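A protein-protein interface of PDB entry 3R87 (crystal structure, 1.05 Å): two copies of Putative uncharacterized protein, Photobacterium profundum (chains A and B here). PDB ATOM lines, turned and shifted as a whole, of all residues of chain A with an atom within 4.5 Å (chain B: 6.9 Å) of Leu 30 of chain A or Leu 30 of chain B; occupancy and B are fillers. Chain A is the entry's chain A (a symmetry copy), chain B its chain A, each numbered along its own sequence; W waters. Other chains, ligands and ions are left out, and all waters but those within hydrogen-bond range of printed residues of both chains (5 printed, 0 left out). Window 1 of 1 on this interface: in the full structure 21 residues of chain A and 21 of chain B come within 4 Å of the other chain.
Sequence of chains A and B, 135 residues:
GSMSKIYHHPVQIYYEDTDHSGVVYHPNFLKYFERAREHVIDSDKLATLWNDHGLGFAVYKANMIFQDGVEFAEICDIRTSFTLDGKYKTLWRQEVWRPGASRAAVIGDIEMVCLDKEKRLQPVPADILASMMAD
The backbone carbonyl oxygen (O) of Ala 62 of chain B is in hydrogen-bond range of the backbone NH (N) of Met 64 of chain A.
The backbone NH of Met 64 of chain B lies within hydrogen-bond range of the backbone carbonyl oxygen of Ala 62 of chain A, 2.8 Å away.
The backbone carbonyl oxygen of Ala 62 of chain A lies close to the backbone carbonyl oxygen of Ala 62 of chain B (3.4 Å).
The side-chain amide nitrogen of Asn 28 of chain B lies close to the backbone carbonyl oxygen of Tyr 25 of chain B.
The guanidinium group (NH1) of Arg 37 of chain B sits at hydrogen-bond distance from the side-chain amide oxygen (OE1) of Gln 94 of chain B (2.9 Å).
Among the printed residues, merely in contact across the chains: Met 64 of chain A with Lys 61 of chain B (3.3 Å), Lys 31 of chain A with Tyr 25 of chain B (3.4 Å), His 26 of chain A with Val 59 of chain B (3.6 Å), Ala 62 of chain A with Asn 63 of chain B (3.6 Å), Lys 31 of chain A with Lys 31 of chain B (3.7 Å), Pro 27 of chain A with Pro 27 of chain B (3.8 Å), Pro 27 of chain A with Leu 30 of chain B (3.8 Å), Leu 30 of chain A with Pro 27 of chain B (3.8 Å), His 26 of chain A with Arg 37 of chain B (3.8 Å), Leu 30 of chain A with Leu 30 of chain B (3.9 Å), Met 64 of chain A with Asn 63 of chain B (3.9 Å), Glu 34 of chain A with Tyr 25 of chain B (3.97 Å), Lys 31 of chain A with Pro 27 of chain B (3.998 Å) and Pro 27 of chain A with Lys 31 of chain B (3.999 Å).
Of the printed residues of chain A, Leu 30 of chain B touches Pro 27 (3.8 Å) and Leu 30 (3.9 Å).
Printed residues of chain B within 4 Å of Ala 62 of chain A: Ala 62 (3.4 Å), Asn 63 (3.6 Å) and Met 64 (2.8 Å).
Printed residues of chain A within 4 Å of Lys 31 of chain B: Pro 27 (3.999 Å) and Lys 31 (3.7 Å).
The nearest printed residue of chain A that does not touch Leu 30 of chain B is His 26 of chain A (4.3 Å).
Of the 12 printed residues of chain A, 7 touch a printed residue of chain B.
Hydrophobic or aromatic side chains of chain A that line the printed part of chain B: His 26, Pro 27, Leu 30 and Met 64.
Of the 22 printed residues of chain B, 10 touch a printed residue of chain A.
Printed residues of chain B that touch a printed residue of chain A: Tyr 25, Pro 27, Leu 30, Lys 31, Arg 37, Val 59, Lys 61, Ala 62, Asn 63 and Met 64.
Hydrophobic or aromatic side chains of chain B that line the printed part of chain A: Tyr 25, Pro 27, Leu 30, Val 59 and Met 64.
Among the printed residues, no Asp or Glu carboxylate lies within 4 Å of a Lys or Arg side-chain nitrogen of the other chain.
Pro 27 of chain A touches Lys 31 of chain B, and with the chains exchanged Lys 31 of chain A touches Pro 27 of chain B.
Positions printed for both chains: 26, 27, 28, 29, 30, 31, 32, 33, 34, 62, 64 and 110.
Water W2 bridges the side-chain carboxylate of Glu 34 of chain A (2.7 Å) and the side-chain hydroxyl of Tyr 25 of chain B (2.7 Å).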
ATOM      1  N   HIS A  26       8.032  -3.204 -10.911  1.00  0.00           N
ATOM      2  CA  HIS A  26       7.608  -4.607 -10.761  1.00  0.00           C
ATOM      3  C   HIS A  26       6.690  -4.904  -9.605  1.00  0.00           C
ATOM      4  O   HIS A  26       5.821  -5.785  -9.748  1.00  0.00           O
ATOM      5  CB  HIS A  26       8.802  -5.565 -10.835  1.00  0.00           C
ATOM      6  CG  HIS A  26       9.699  -5.525  -9.627  1.00  0.00           C
ATOM      7  ND1 HIS A  26      10.728  -4.633  -9.502  1.00  0.00           N
ATOM      8  CD2 HIS A  26       9.685  -6.245  -8.474  1.00  0.00           C
ATOM      9  CE1 HIS A  26      11.283  -4.810  -8.301  1.00  0.00           C
ATOM     10  NE2 HIS A  26      10.688  -5.759  -7.622  1.00  0.00           N
ATOM     11  N   PRO A  27       6.804  -4.276  -8.410  1.00  0.00           N
ATOM     12  CA  PRO A  27       5.867  -4.604  -7.340  1.00  0.00           C
ATOM     13  C   PRO A  27       4.428  -4.359  -7.706  1.00  0.00           C
ATOM     14  O   PRO A  27       3.489  -4.972  -7.159  1.00  0.00           O
ATOM     15  CB  PRO A  27       6.305  -3.740  -6.178  1.00  0.00           C
ATOM     16  CG  PRO A  27       7.782  -3.562  -6.438  1.00  0.00           C
ATOM     17  CD  PRO A  27       7.868  -3.355  -7.937  1.00  0.00           C
ATOM     18  N   ASN A  28       4.184  -3.458  -8.675  1.00  0.00           N
ATOM     19  CA  ASN A  28       2.798  -3.148  -9.030  1.00  0.00           C
ATOM     20  C   ASN A  28       2.067  -4.341  -9.624  1.00  0.00           C
ATOM     21  O   ASN A  28       0.842  -4.395  -9.535  1.00  0.00           O
ATOM     22  CB  ASN A  28       2.777  -1.977 -10.021  1.00  0.00           C
ATOM     23  CG  ASN A  28       3.235  -0.692  -9.365  1.00  0.00           C
ATOM     24  OD1 ASN A  28       3.149  -0.548  -8.143  1.00  0.00           O
ATOM     25  ND2 ASN A  28       3.757   0.226 -10.141  1.00  0.00           N
ATOM     26  N   PHE A  29       2.785  -5.298 -10.236  1.00  0.00           N
ATOM     27  CA  PHE A  29       2.081  -6.434 -10.804  1.00  0.00           C
ATOM     28  C   PHE A  29       1.319  -7.214  -9.758  1.00  0.00           C
ATOM     29  O   PHE A  29       0.237  -7.773 -10.054  1.00  0.00           O
ATOM     30  CB  PHE A  29       3.039  -7.313 -11.604  1.00  0.00           C
ATOM     31  CG  PHE A  29       3.600  -6.643 -12.799  1.00  0.00           C
ATOM     32  CD1 PHE A  29       2.776  -6.242 -13.870  1.00  0.00           C
ATOM     33  CD2 PHE A  29       4.951  -6.358 -12.906  1.00  0.00           C
ATOM     34  CE1 PHE A  29       3.287  -5.672 -14.988  1.00  0.00           C
ATOM     35  CE2 PHE A  29       5.482  -5.777 -14.042  1.00  0.00           C
ATOM     36  CZ  PHE A  29       4.658  -5.432 -15.116  1.00  0.00           C
ATOM     37  N   LEU A  30       1.842  -7.325  -8.529  1.00  0.00           N
ATOM     38  CA  LEU A  30       1.084  -8.008  -7.503  1.00  0.00           C
ATOM     39  C   LEU A  30      -0.174  -7.278  -7.124  1.00  0.00           C
ATOM     40  O   LEU A  30      -1.166  -7.903  -6.716  1.00  0.00           O
ATOM     41  CB  LEU A  30       1.896  -8.340  -6.248  1.00  0.00           C
ATOM     42  CG  LEU A  30       2.750  -9.607  -6.284  1.00  0.00           C
ATOM     43  CD1 LEU A  30       3.788  -9.373  -5.129  1.00  0.00           C
ATOM     44  CD2 LEU A  30       1.919 -10.890  -6.274  1.00  0.00           C
ATOM     45  N   LYS A  31      -0.178  -5.933  -7.259  1.00  0.00           N
ATOM     46  CA  LYS A  31      -1.430  -5.189  -7.054  1.00  0.00           C
ATOM     47  C   LYS A  31      -2.481  -5.612  -8.100  1.00  0.00           C
ATOM     48  O   LYS A  31      -3.655  -5.806  -7.766  1.00  0.00           O
ATOM     49  CB  LYS A  31      -1.188  -3.672  -7.174  1.00  0.00           C
ATOM     50  CG  LYS A  31      -0.258  -3.136  -6.150  1.00  0.00           C
ATOM     51  CD  LYS A  31       0.006  -1.649  -6.339  1.00  0.00           C
ATOM     52  CE  LYS A  31       0.989  -1.135  -5.257  1.00  0.00           C
ATOM     53  NZ  LYS A  31       0.907   0.358  -5.021  1.00  0.00           N
ATOM     54  N   TYR A  32      -2.044  -5.686  -9.371  1.00  0.00           N
ATOM     55  CA  TYR A  32      -2.990  -6.029 -10.418  1.00  0.00           C
ATOM     56  C   TYR A  32      -3.537  -7.441 -10.198  1.00  0.00           C
ATOM     57  O   TYR A  32      -4.711  -7.689 -10.438  1.00  0.00           O
ATOM     58  CB  TYR A  32      -2.318  -5.979 -11.780  1.00  0.00           C
ATOM     59  CG  TYR A  32      -1.592  -4.663 -12.089  1.00  0.00           C
ATOM     60  CD1 TYR A  32      -1.911  -3.444 -11.471  1.00  0.00           C
ATOM     61  CD2 TYR A  32      -0.542  -4.694 -12.987  1.00  0.00           C
ATOM     62  CE1 TYR A  32      -1.148  -2.318 -11.734  1.00  0.00           C
ATOM     63  CE2 TYR A  32       0.222  -3.564 -13.267  1.00  0.00           C
ATOM     64  CZ  TYR A  32      -0.086  -2.376 -12.598  1.00  0.00           C
ATOM     65  OH  TYR A  32       0.722  -1.305 -12.835  1.00  0.00           O
ATOM     66  N   PHE A  33      -2.669  -8.362  -9.737  1.00  0.00           N
ATOM     67  CA  PHE A  33      -3.114  -9.699  -9.444  1.00  0.00           C
ATOM     68  C   PHE A  33      -4.140  -9.701  -8.325  1.00  0.00           C
ATOM     69  O   PHE A  33      -5.108 -10.451  -8.368  1.00  0.00           O
ATOM     70  CB  PHE A  33      -1.952 -10.602  -9.144  1.00  0.00           C
ATOM     71  CG  PHE A  33      -1.065 -10.957 -10.303  1.00  0.00           C
ATOM     72  CD1 PHE A  33      -1.422 -10.733 -11.629  1.00  0.00           C
ATOM     73  CD2 PHE A  33       0.144 -11.603 -10.080  1.00  0.00           C
ATOM     74  CE1 PHE A  33      -0.649 -11.151 -12.684  1.00  0.00           C
ATOM     75  CE2 PHE A  33       0.937 -12.017 -11.159  1.00  0.00           C
ATOM     76  CZ  PHE A  33       0.554 -11.785 -12.456  1.00  0.00           C
ATOM     77  N   GLU A  34      -3.933  -8.857  -7.294  1.00  0.00           N
ATOM     78  CA  GLU A  34      -4.882  -8.732  -6.205  1.00  0.00           C
ATOM     79  C   GLU A  34      -6.248  -8.268  -6.736  1.00  0.00           C
ATOM     80  O   GLU A  34      -7.283  -8.851  -6.368  1.00  0.00           O
ATOM     81  CB  GLU A  34      -4.337  -7.800  -5.129  1.00  0.00           C
ATOM     82  CG  GLU A  34      -5.074  -7.872  -3.818  1.00  0.00           C
ATOM     83  CD  GLU A  34      -6.456  -7.168  -3.791  1.00  0.00           C
ATOM     84  OE1 GLU A  34      -6.627  -6.167  -4.423  1.00  0.00           O
ATOM     85  OE2 GLU A  34      -7.371  -7.613  -3.064  1.00  0.00           O
ATOM     86  N   ALA A  62       4.029 -16.227  -3.140  1.00  0.00           N
ATOM     87  CA  ALA A  62       3.914 -15.677  -4.498  1.00  0.00           C
ATOM     88  C   ALA A  62       5.214 -15.932  -5.205  1.00  0.00           C
ATOM     89  O   ALA A  62       6.252 -15.368  -4.796  1.00  0.00           O
ATOM     90  CB  ALA A  62       3.565 -14.212  -4.497  1.00  0.00           C
ATOM     91  N   MET A  64       6.929 -15.279  -8.672  1.00  0.00           N
ATOM     92  CA  MET A  64       6.785 -14.350  -9.793  1.00  0.00           C
ATOM     93  C   MET A  64       7.906 -14.540 -10.791  1.00  0.00           C
ATOM     94  O   MET A  64       9.092 -14.696 -10.397  1.00  0.00           O
ATOM     95  CB  MET A  64       6.808 -12.893  -9.248  1.00  0.00           C
ATOM     96  CG  MET A  64       5.766 -12.524  -8.200  1.00  0.00           C
ATOM     97  SD  MET A  64       4.072 -12.488  -8.801  1.00  0.00           S
ATOM     98  CE  MET A  64       4.132 -11.007  -9.820  1.00  0.00           C
ATOM     99  N   ILE A 110       0.394 -18.080  -6.989  1.00  0.00           N
ATOM    100  CA  ILE A 110       0.046 -17.491  -5.708  1.00  0.00           C
ATOM    101  C   ILE A 110      -0.682 -18.475  -4.849  1.00  0.00           C
ATOM    102  O   ILE A 110      -1.580 -19.187  -5.336  1.00  0.00           O
ATOM    103  CB  ILE A 110      -0.756 -16.196  -5.890  1.00  0.00           C
ATOM    104  CG1 ILE A 110       0.115 -14.963  -6.193  1.00  0.00           C
ATOM    105  CG2 ILE A 110      -1.607 -15.939  -4.657  1.00  0.00           C
ATOM    106  CD1 ILE A 110       0.808 -14.853  -7.073  1.00  0.00           C
ATOM    107  N   TYR B  25       0.315  -4.066   3.393  1.00  0.00           N
ATOM    108  CA  TYR B  25      -0.207  -4.573   2.144  1.00  0.00           C
ATOM    109  C   TYR B  25       0.924  -5.295   1.404  1.00  0.00           C
ATOM    110  O   TYR B  25       1.978  -4.681   1.141  1.00  0.00           O
ATOM    111  CB  TYR B  25      -0.787  -3.360   1.381  1.00  0.00           C
ATOM    112  CG  TYR B  25      -1.279  -3.693  -0.005  1.00  0.00           C
ATOM    113  CD1 TYR B  25      -2.264  -4.604  -0.220  1.00  0.00           C
ATOM    114  CD2 TYR B  25      -0.741  -2.999  -1.105  1.00  0.00           C
ATOM    115  CE1 TYR B  25      -2.676  -4.876  -1.586  1.00  0.00           C
ATOM    116  CE2 TYR B  25      -1.145  -3.256  -2.408  1.00  0.00           C
ATOM    117  CZ  TYR B  25      -2.102  -4.212  -2.604  1.00  0.00           C
ATOM    118  OH  TYR B  25      -2.439  -4.531  -3.922  1.00  0.00           O
ATOM    119  N   HIS B  26       0.728  -6.566   1.042  1.00  0.00           N
ATOM    120  CA  HIS B  26       1.870  -7.429   0.694  1.00  0.00           C
ATOM    121  C   HIS B  26       2.734  -6.961  -0.448  1.00  0.00           C
ATOM    122  O   HIS B  26       3.956  -7.195  -0.402  1.00  0.00           O
ATOM    123  CB  HIS B  26       1.444  -8.896   0.555  1.00  0.00           C
ATOM    124  CG  HIS B  26       0.626  -9.186  -0.675  1.00  0.00           C
ATOM    125  ND1 HIS B  26      -0.732  -9.035  -0.708  1.00  0.00           N
ATOM    126  CD2 HIS B  26       0.992  -9.574  -1.925  1.00  0.00           C
ATOM    127  CE1 HIS B  26      -1.146  -9.305  -1.949  1.00  0.00           C
ATOM    128  NE2 HIS B  26      -0.150  -9.622  -2.739  1.00  0.00           N
ATOM    129  N   PRO B  27       2.222  -6.331  -1.531  1.00  0.00           N
ATOM    130  CA  PRO B  27       3.123  -5.890  -2.592  1.00  0.00           C
ATOM    131  C   PRO B  27       4.179  -4.928  -2.120  1.00  0.00           C
ATOM    132  O   PRO B  27       5.271  -4.798  -2.709  1.00  0.00           O
ATOM    133  CB  PRO B  27       2.211  -5.261  -3.623  1.00  0.00           C
ATOM    134  CG  PRO B  27       0.913  -6.004  -3.413  1.00  0.00           C
ATOM    135  CD  PRO B  27       0.800  -6.123  -1.906  1.00  0.00           C
ATOM    136  N   ASN B  28       3.912  -4.216  -1.010  1.00  0.00           N
ATOM    137  CA  ASN B  28       4.887  -3.230  -0.541  1.00  0.00           C
ATOM    138  C   ASN B  28       6.198  -3.867  -0.107  1.00  0.00           C
ATOM    139  O   ASN B  28       7.228  -3.195  -0.143  1.00  0.00           O
ATOM    140  CB  ASN B  28       4.285  -2.432   0.623  1.00  0.00           C
ATOM    141  CG  ASN B  28       3.141  -1.556   0.156  1.00  0.00           C
ATOM    142  OD1 ASN B  28       3.068  -1.198  -1.022  1.00  0.00           O
ATOM    143  ND2 ASN B  28       2.228  -1.239   1.040  1.00  0.00           N
ATOM    144  N   PHE B  29       6.188  -5.143   0.308  1.00  0.00           N
ATOM    145  CA  PHE B  29       7.443  -5.746   0.724  1.00  0.00           C
ATOM    146  C   PHE B  29       8.460  -5.772  -0.392  1.00  0.00           C
ATOM    147  O   PHE B  29       9.681  -5.650  -0.135  1.00  0.00           O
ATOM    148  CB  PHE B  29       7.201  -7.127   1.325  1.00  0.00           C
ATOM    149  CG  PHE B  29       6.418  -7.098   2.582  1.00  0.00           C
ATOM    150  CD1 PHE B  29       6.918  -6.474   3.742  1.00  0.00           C
ATOM    151  CD2 PHE B  29       5.155  -7.659   2.665  1.00  0.00           C
ATOM    152  CE1 PHE B  29       6.229  -6.484   4.910  1.00  0.00           C
ATOM    153  CE2 PHE B  29       4.445  -7.674   3.850  1.00  0.00           C
ATOM    154  CZ  PHE B  29       4.976  -7.096   5.006  1.00  0.00           C
ATOM    155  N   LEU B  30       8.034  -5.966  -1.649  1.00  0.00           N
ATOM    156  CA  LEU B  30       8.994  -5.921  -2.730  1.00  0.00           C
ATOM    157  C   LEU B  30       9.587  -4.553  -2.925  1.00  0.00           C
ATOM    158  O   LEU B  30      10.736  -4.424  -3.377  1.00  0.00           O
ATOM    159  CB  LEU B  30       8.456  -6.453  -4.062  1.00  0.00           C
ATOM    160  CG  LEU B  30       8.484  -7.967  -4.269  1.00  0.00           C
ATOM    161  CD1 LEU B  30       7.441  -8.189  -5.423  1.00  0.00           C
ATOM    162  CD2 LEU B  30       9.897  -8.523  -4.439  1.00  0.00           C
ATOM    163  N   LYS B  31       8.828  -3.490  -2.579  1.00  0.00           N
ATOM    164  CA  LYS B  31       9.418  -2.142  -2.601  1.00  0.00           C
ATOM    165  C   LYS B  31      10.573  -2.048  -1.583  1.00  0.00           C
ATOM    166  O   LYS B  31      11.628  -1.478  -1.885  1.00  0.00           O
ATOM    167  CB  LYS B  31       8.358  -1.078  -2.255  1.00  0.00           C
ATOM    168  CG  LYS B  31       7.239  -1.017  -3.226  1.00  0.00           C
ATOM    169  CD  LYS B  31       6.181  -0.002  -2.818  1.00  0.00           C
ATOM    170  CE  LYS B  31       5.028   0.022  -3.852  1.00  0.00           C
ATOM    171  NZ  LYS B  31       4.230   1.307  -3.845  1.00  0.00           N
ATOM    172  N   TYR B  32      10.320  -2.558  -0.364  1.00  0.00           N
ATOM    173  CA  TYR B  32      11.344  -2.458   0.661  1.00  0.00           C
ATOM    174  C   TYR B  32      12.588  -3.247   0.249  1.00  0.00           C
ATOM    175  O   TYR B  32      13.704  -2.813   0.505  1.00  0.00           O
ATOM    176  CB  TYR B  32      10.832  -3.018   1.979  1.00  0.00           C
ATOM    177  CG  TYR B  32       9.502  -2.423   2.456  1.00  0.00           C
ATOM    178  CD1 TYR B  32       9.035  -1.161   2.055  1.00  0.00           C
ATOM    179  CD2 TYR B  32       8.705  -3.191   3.284  1.00  0.00           C
ATOM    180  CE1 TYR B  32       7.780  -0.734   2.455  1.00  0.00           C
ATOM    181  CE2 TYR B  32       7.447  -2.762   3.701  1.00  0.00           C
ATOM    182  CZ  TYR B  32       6.987  -1.524   3.244  1.00  0.00           C
ATOM    183  OH  TYR B  32       5.724  -1.163   3.606  1.00  0.00           O
ATOM    184  N   PHE B  33      12.381  -4.411  -0.394  1.00  0.00           N
ATOM    185  CA  PHE B  33      13.496  -5.188  -0.873  1.00  0.00           C
ATOM    186  C   PHE B  33      14.280  -4.425  -1.925  1.00  0.00           C
ATOM    187  O   PHE B  33      15.504  -4.482  -1.953  1.00  0.00           O
ATOM    188  CB  PHE B  33      13.045  -6.532  -1.370  1.00  0.00           C
ATOM    189  CG  PHE B  33      12.580  -7.507  -0.328  1.00  0.00           C
ATOM    190  CD1 PHE B  33      12.811  -7.333   1.033  1.00  0.00           C
ATOM    191  CD2 PHE B  33      11.949  -8.684  -0.710  1.00  0.00           C
ATOM    192  CE1 PHE B  33      12.470  -8.279   1.969  1.00  0.00           C
ATOM    193  CE2 PHE B  33      11.591  -9.641   0.249  1.00  0.00           C
ATOM    194  CZ  PHE B  33      11.836  -9.441   1.583  1.00  0.00           C
ATOM    195  N   GLU B  34      13.577  -3.701  -2.819  1.00  0.00           N
ATOM    196  CA  GLU B  34      14.227  -2.885  -3.825  1.00  0.00           C
ATOM    197  C   GLU B  34      15.107  -1.815  -3.160  1.00  0.00           C
ATOM    198  O   GLU B  34      16.269  -1.634  -3.564  1.00  0.00           O
ATOM    199  CB  GLU B  34      13.193  -2.277  -4.766  1.00  0.00           C
ATOM    200  CG  GLU B  34      13.773  -1.706  -6.034  1.00  0.00           C
ATOM    201  CD  GLU B  34      14.501  -0.344  -5.879  1.00  0.00           C
ATOM    202  OE1 GLU B  34      14.099   0.459  -5.090  1.00  0.00           O
ATOM    203  OE2 GLU B  34      15.468  -0.065  -6.621  1.00  0.00           O
ATOM    204  N   ARG B  35      14.574  -1.116  -2.163  1.00  0.00           N
ATOM    205  CA  ARG B  35      15.349  -0.092  -1.480  1.00  0.00           C
ATOM    206  C   ARG B  35      16.620  -0.697  -0.926  1.00  0.00           C
ATOM    207  O   ARG B  35      17.712  -0.131  -1.006  1.00  0.00           O
ATOM    208  CB  ARG B  35      14.552   0.517  -0.325  1.00  0.00           C
ATOM    209  CG  ARG B  35      13.259   1.197  -0.704  1.00  0.00           C
ATOM    210  CD  ARG B  35      12.567   1.685   0.547  1.00  0.00           C
ATOM    211  NE  ARG B  35      11.185   2.036   0.293  1.00  0.00           N
ATOM    212  CZ  ARG B  35      10.285   2.289   1.230  1.00  0.00           C
ATOM    213  NH1 ARG B  35      10.665   2.287   2.513  1.00  0.00           N
ATOM    214  NH2 ARG B  35       9.027   2.470   0.897  1.00  0.00           N
ATOM    215  N   ARG B  37      18.295  -3.399  -1.768  1.00  0.00           N
ATOM    216  CA  ARG B  37      19.285  -3.696  -2.784  1.00  0.00           C
ATOM    217  C   ARG B  37      20.007  -2.441  -3.228  1.00  0.00           C
ATOM    218  O   ARG B  37      21.221  -2.472  -3.461  1.00  0.00           O
ATOM    219  CB  ARG B  37      18.689  -4.414  -3.983  1.00  0.00           C
ATOM    220  CG  ARG B  37      18.116  -5.769  -3.682  1.00  0.00           C
ATOM    221  CD  ARG B  37      17.736  -6.563  -4.930  1.00  0.00           C
ATOM    222  NE  ARG B  37      16.740  -5.872  -5.754  1.00  0.00           N
ATOM    223  CZ  ARG B  37      15.423  -5.969  -5.592  1.00  0.00           C
ATOM    224  NH1 ARG B  37      14.883  -6.705  -4.662  1.00  0.00           N
ATOM    225  NH2 ARG B  37      14.617  -5.306  -6.446  1.00  0.00           N
ATOM    226  N   VAL B  59      14.355  -7.210 -11.956  1.00  0.00           N
ATOM    227  CA  VAL B  59      14.021  -8.443 -11.304  1.00  0.00           C
ATOM    228  C   VAL B  59      13.464  -9.386 -12.352  1.00  0.00           C
ATOM    229  O   VAL B  59      12.455  -9.063 -13.011  1.00  0.00           O
ATOM    230  CB  VAL B  59      13.038  -8.195 -10.133  1.00  0.00           C
ATOM    231  CG1 VAL B  59      12.549  -9.489  -9.576  1.00  0.00           C
ATOM    232  CG2 VAL B  59      13.676  -7.337  -9.011  1.00  0.00           C
ATOM    233  N   LYS B  61      13.044 -12.951 -11.355  1.00  0.00           N
ATOM    234  CA  LYS B  61      12.241 -13.852 -10.556  1.00  0.00           C
ATOM    235  C   LYS B  61      12.207 -13.336  -9.136  1.00  0.00           C
ATOM    236  O   LYS B  61      13.213 -12.824  -8.628  1.00  0.00           O
ATOM    237  CB  LYS B  61      12.762 -15.293 -10.580  1.00  0.00           C
ATOM    238  CG  LYS B  61      12.479 -15.959 -11.899  1.00  0.00           C
ATOM    239  CD  LYS B  61      12.916 -17.441 -11.875  1.00  0.00           C
ATOM    240  CE  LYS B  61      12.548 -18.144 -13.172  1.00  0.00           C
ATOM    241  NZ  LYS B  61      12.953 -19.572 -13.084  1.00  0.00           N
ATOM    242  N   ALA B  62      11.064 -13.530  -8.481  1.00  0.00           N
ATOM    243  CA  ALA B  62      10.912 -13.236  -7.049  1.00  0.00           C
ATOM    244  C   ALA B  62      10.028 -14.297  -6.457  1.00  0.00           C
ATOM    245  O   ALA B  62       8.836 -14.372  -6.824  1.00  0.00           O
ATOM    246  CB  ALA B  62      10.360 -11.857  -6.801  1.00  0.00           C
ATOM    247  N   ASN B  63      10.560 -15.071  -5.530  1.00  0.00           N
ATOM    248  CA  ASN B  63       9.804 -16.107  -4.826  1.00  0.00           C
ATOM    249  C   ASN B  63       9.625 -15.635  -3.414  1.00  0.00           C
ATOM    250  O   ASN B  63      10.647 -15.545  -2.671  1.00  0.00           O
ATOM    251  CB  ASN B  63      10.468 -17.478  -4.858  1.00  0.00           C
ATOM    252  CG  ASN B  63      10.473 -18.059  -6.252  1.00  0.00           C
ATOM    253  OD1 ASN B  63       9.758 -17.571  -7.152  1.00  0.00           O
ATOM    254  ND2 ASN B  63      10.955 -19.172  -6.380  1.00  0.00           N
ATOM    255  N   MET B  64       8.425 -15.300  -3.021  1.00  0.00           N
ATOM    256  CA  MET B  64       8.068 -14.648  -1.762  1.00  0.00           C
ATOM    257  C   MET B  64       7.308 -15.600  -0.864  1.00  0.00           C
ATOM    258  O   MET B  64       6.407 -16.342  -1.337  1.00  0.00           O
ATOM    259  CB  MET B  64       7.188 -13.402  -2.069  1.00  0.00           C
ATOM    260  CG  MET B  64       7.778 -12.344  -2.993  1.00  0.00           C
ATOM    261  SD  MET B  64       9.175 -11.440  -2.309  1.00  0.00           S
ATOM    262  CE  MET B  64       8.330 -10.444  -1.073  1.00  0.00           C
ATOM    263  N   PHE B  66       5.177 -14.994   2.791  1.00  0.00           N
ATOM    264  CA  PHE B  66       4.631 -14.003   3.716  1.00  0.00           C
ATOM    265  C   PHE B  66       4.154 -14.789   4.914  1.00  0.00           C
ATOM    266  O   PHE B  66       3.110 -15.432   4.843  1.00  0.00           O
ATOM    267  CB  PHE B  66       3.518 -13.182   3.089  1.00  0.00           C
ATOM    268  CG  PHE B  66       3.881 -12.533   1.794  1.00  0.00           C
ATOM    269  CD1 PHE B  66       4.482 -11.289   1.709  1.00  0.00           C
ATOM    270  CD2 PHE B  66       3.632 -13.211   0.597  1.00  0.00           C
ATOM    271  CE1 PHE B  66       4.806 -10.723   0.482  1.00  0.00           C
ATOM    272  CE2 PHE B  66       3.926 -12.640  -0.606  1.00  0.00           C
ATOM    273  CZ  PHE B  66       4.514 -11.392  -0.715  1.00  0.00           C
ATOM    274  N   GLN B  94      16.443 -11.931   0.765  1.00  0.00           N
ATOM    275  CA  GLN B  94      16.013 -10.767   1.476  1.00  0.00           C
ATOM    276  C   GLN B  94      14.931 -11.133   2.445  1.00  0.00           C
ATOM    277  O   GLN B  94      14.029 -11.936   2.118  1.00  0.00           O
ATOM    278  CB  GLN B  94      15.576  -9.631   0.535  1.00  0.00           C
ATOM    279  CG  GLN B  94      16.663  -9.306  -0.474  1.00  0.00           C
ATOM    280  CD  GLN B  94      16.382  -8.040  -1.230  1.00  0.00           C
ATOM    281  OE1 GLN B  94      15.863  -8.093  -2.357  1.00  0.00           O
ATOM    282  NE2 GLN B  94      16.657  -6.901  -0.615  1.00  0.00           N
ATOM    283  N   VAL B 106       8.702 -11.989   6.312  1.00  0.00           N
ATOM    284  CA  VAL B 106       8.635 -12.083   4.854  1.00  0.00           C
ATOM    285  C   VAL B 106       9.996 -12.547   4.380  1.00  0.00           C
ATOM    286  O   VAL B 106      11.025 -12.014   4.854  1.00  0.00           O
ATOM    287  CB  VAL B 106       8.239 -10.765   4.198  1.00  0.00           C
ATOM    288  CG1 VAL B 106       8.163 -10.910   2.666  1.00  0.00           C
ATOM    289  CG2 VAL B 106       6.951 -10.225   4.771  1.00  0.00           C
ATOM    290  N   GLY B 108      12.158 -13.356   0.663  1.00  0.00           N
ATOM    291  CA  GLY B 108      12.222 -13.322  -0.790  1.00  0.00           C
ATOM    292  C   GLY B 108      13.525 -13.895  -1.281  1.00  0.00           C
ATOM    293  O   GLY B 108      14.614 -13.565  -0.768  1.00  0.00           O
ATOM    294  N   ILE B 110      15.294 -13.551  -4.797  1.00  0.00           N
ATOM    295  CA  ILE B 110      15.177 -12.676  -5.949  1.00  0.00           C
ATOM    296  C   ILE B 110      16.293 -12.914  -6.915  1.00  0.00           C
ATOM    297  O   ILE B 110      17.460 -13.052  -6.502  1.00  0.00           O
ATOM    298  CB  ILE B 110      15.102 -11.203  -5.524  1.00  0.00           C
ATOM    299  CG1 ILE B 110      13.699 -10.756  -5.073  1.00  0.00           C
ATOM    300  CG2 ILE B 110      15.590 -10.315  -6.657  1.00  0.00           C
ATOM    301  CD1 ILE B 110      13.112 -11.203  -4.224  1.00  0.00           C
HETATM  302  O   HOH W   1      -1.223 -10.281  -5.209  1.00  0.00           O
HETATM  303  O   HOH W   2      -5.006  -4.053  -4.453  1.00  0.00           O
HETATM  304  O   HOH W   3      12.067  -6.067  -5.236  1.00  0.00           O
HETATM  305  O   HOH W   4      12.464  -5.008 -12.376  1.00  0.00           O
HETATM  306  O   HOH W   5       9.760 -17.369  -9.781  1.00  0.00           O
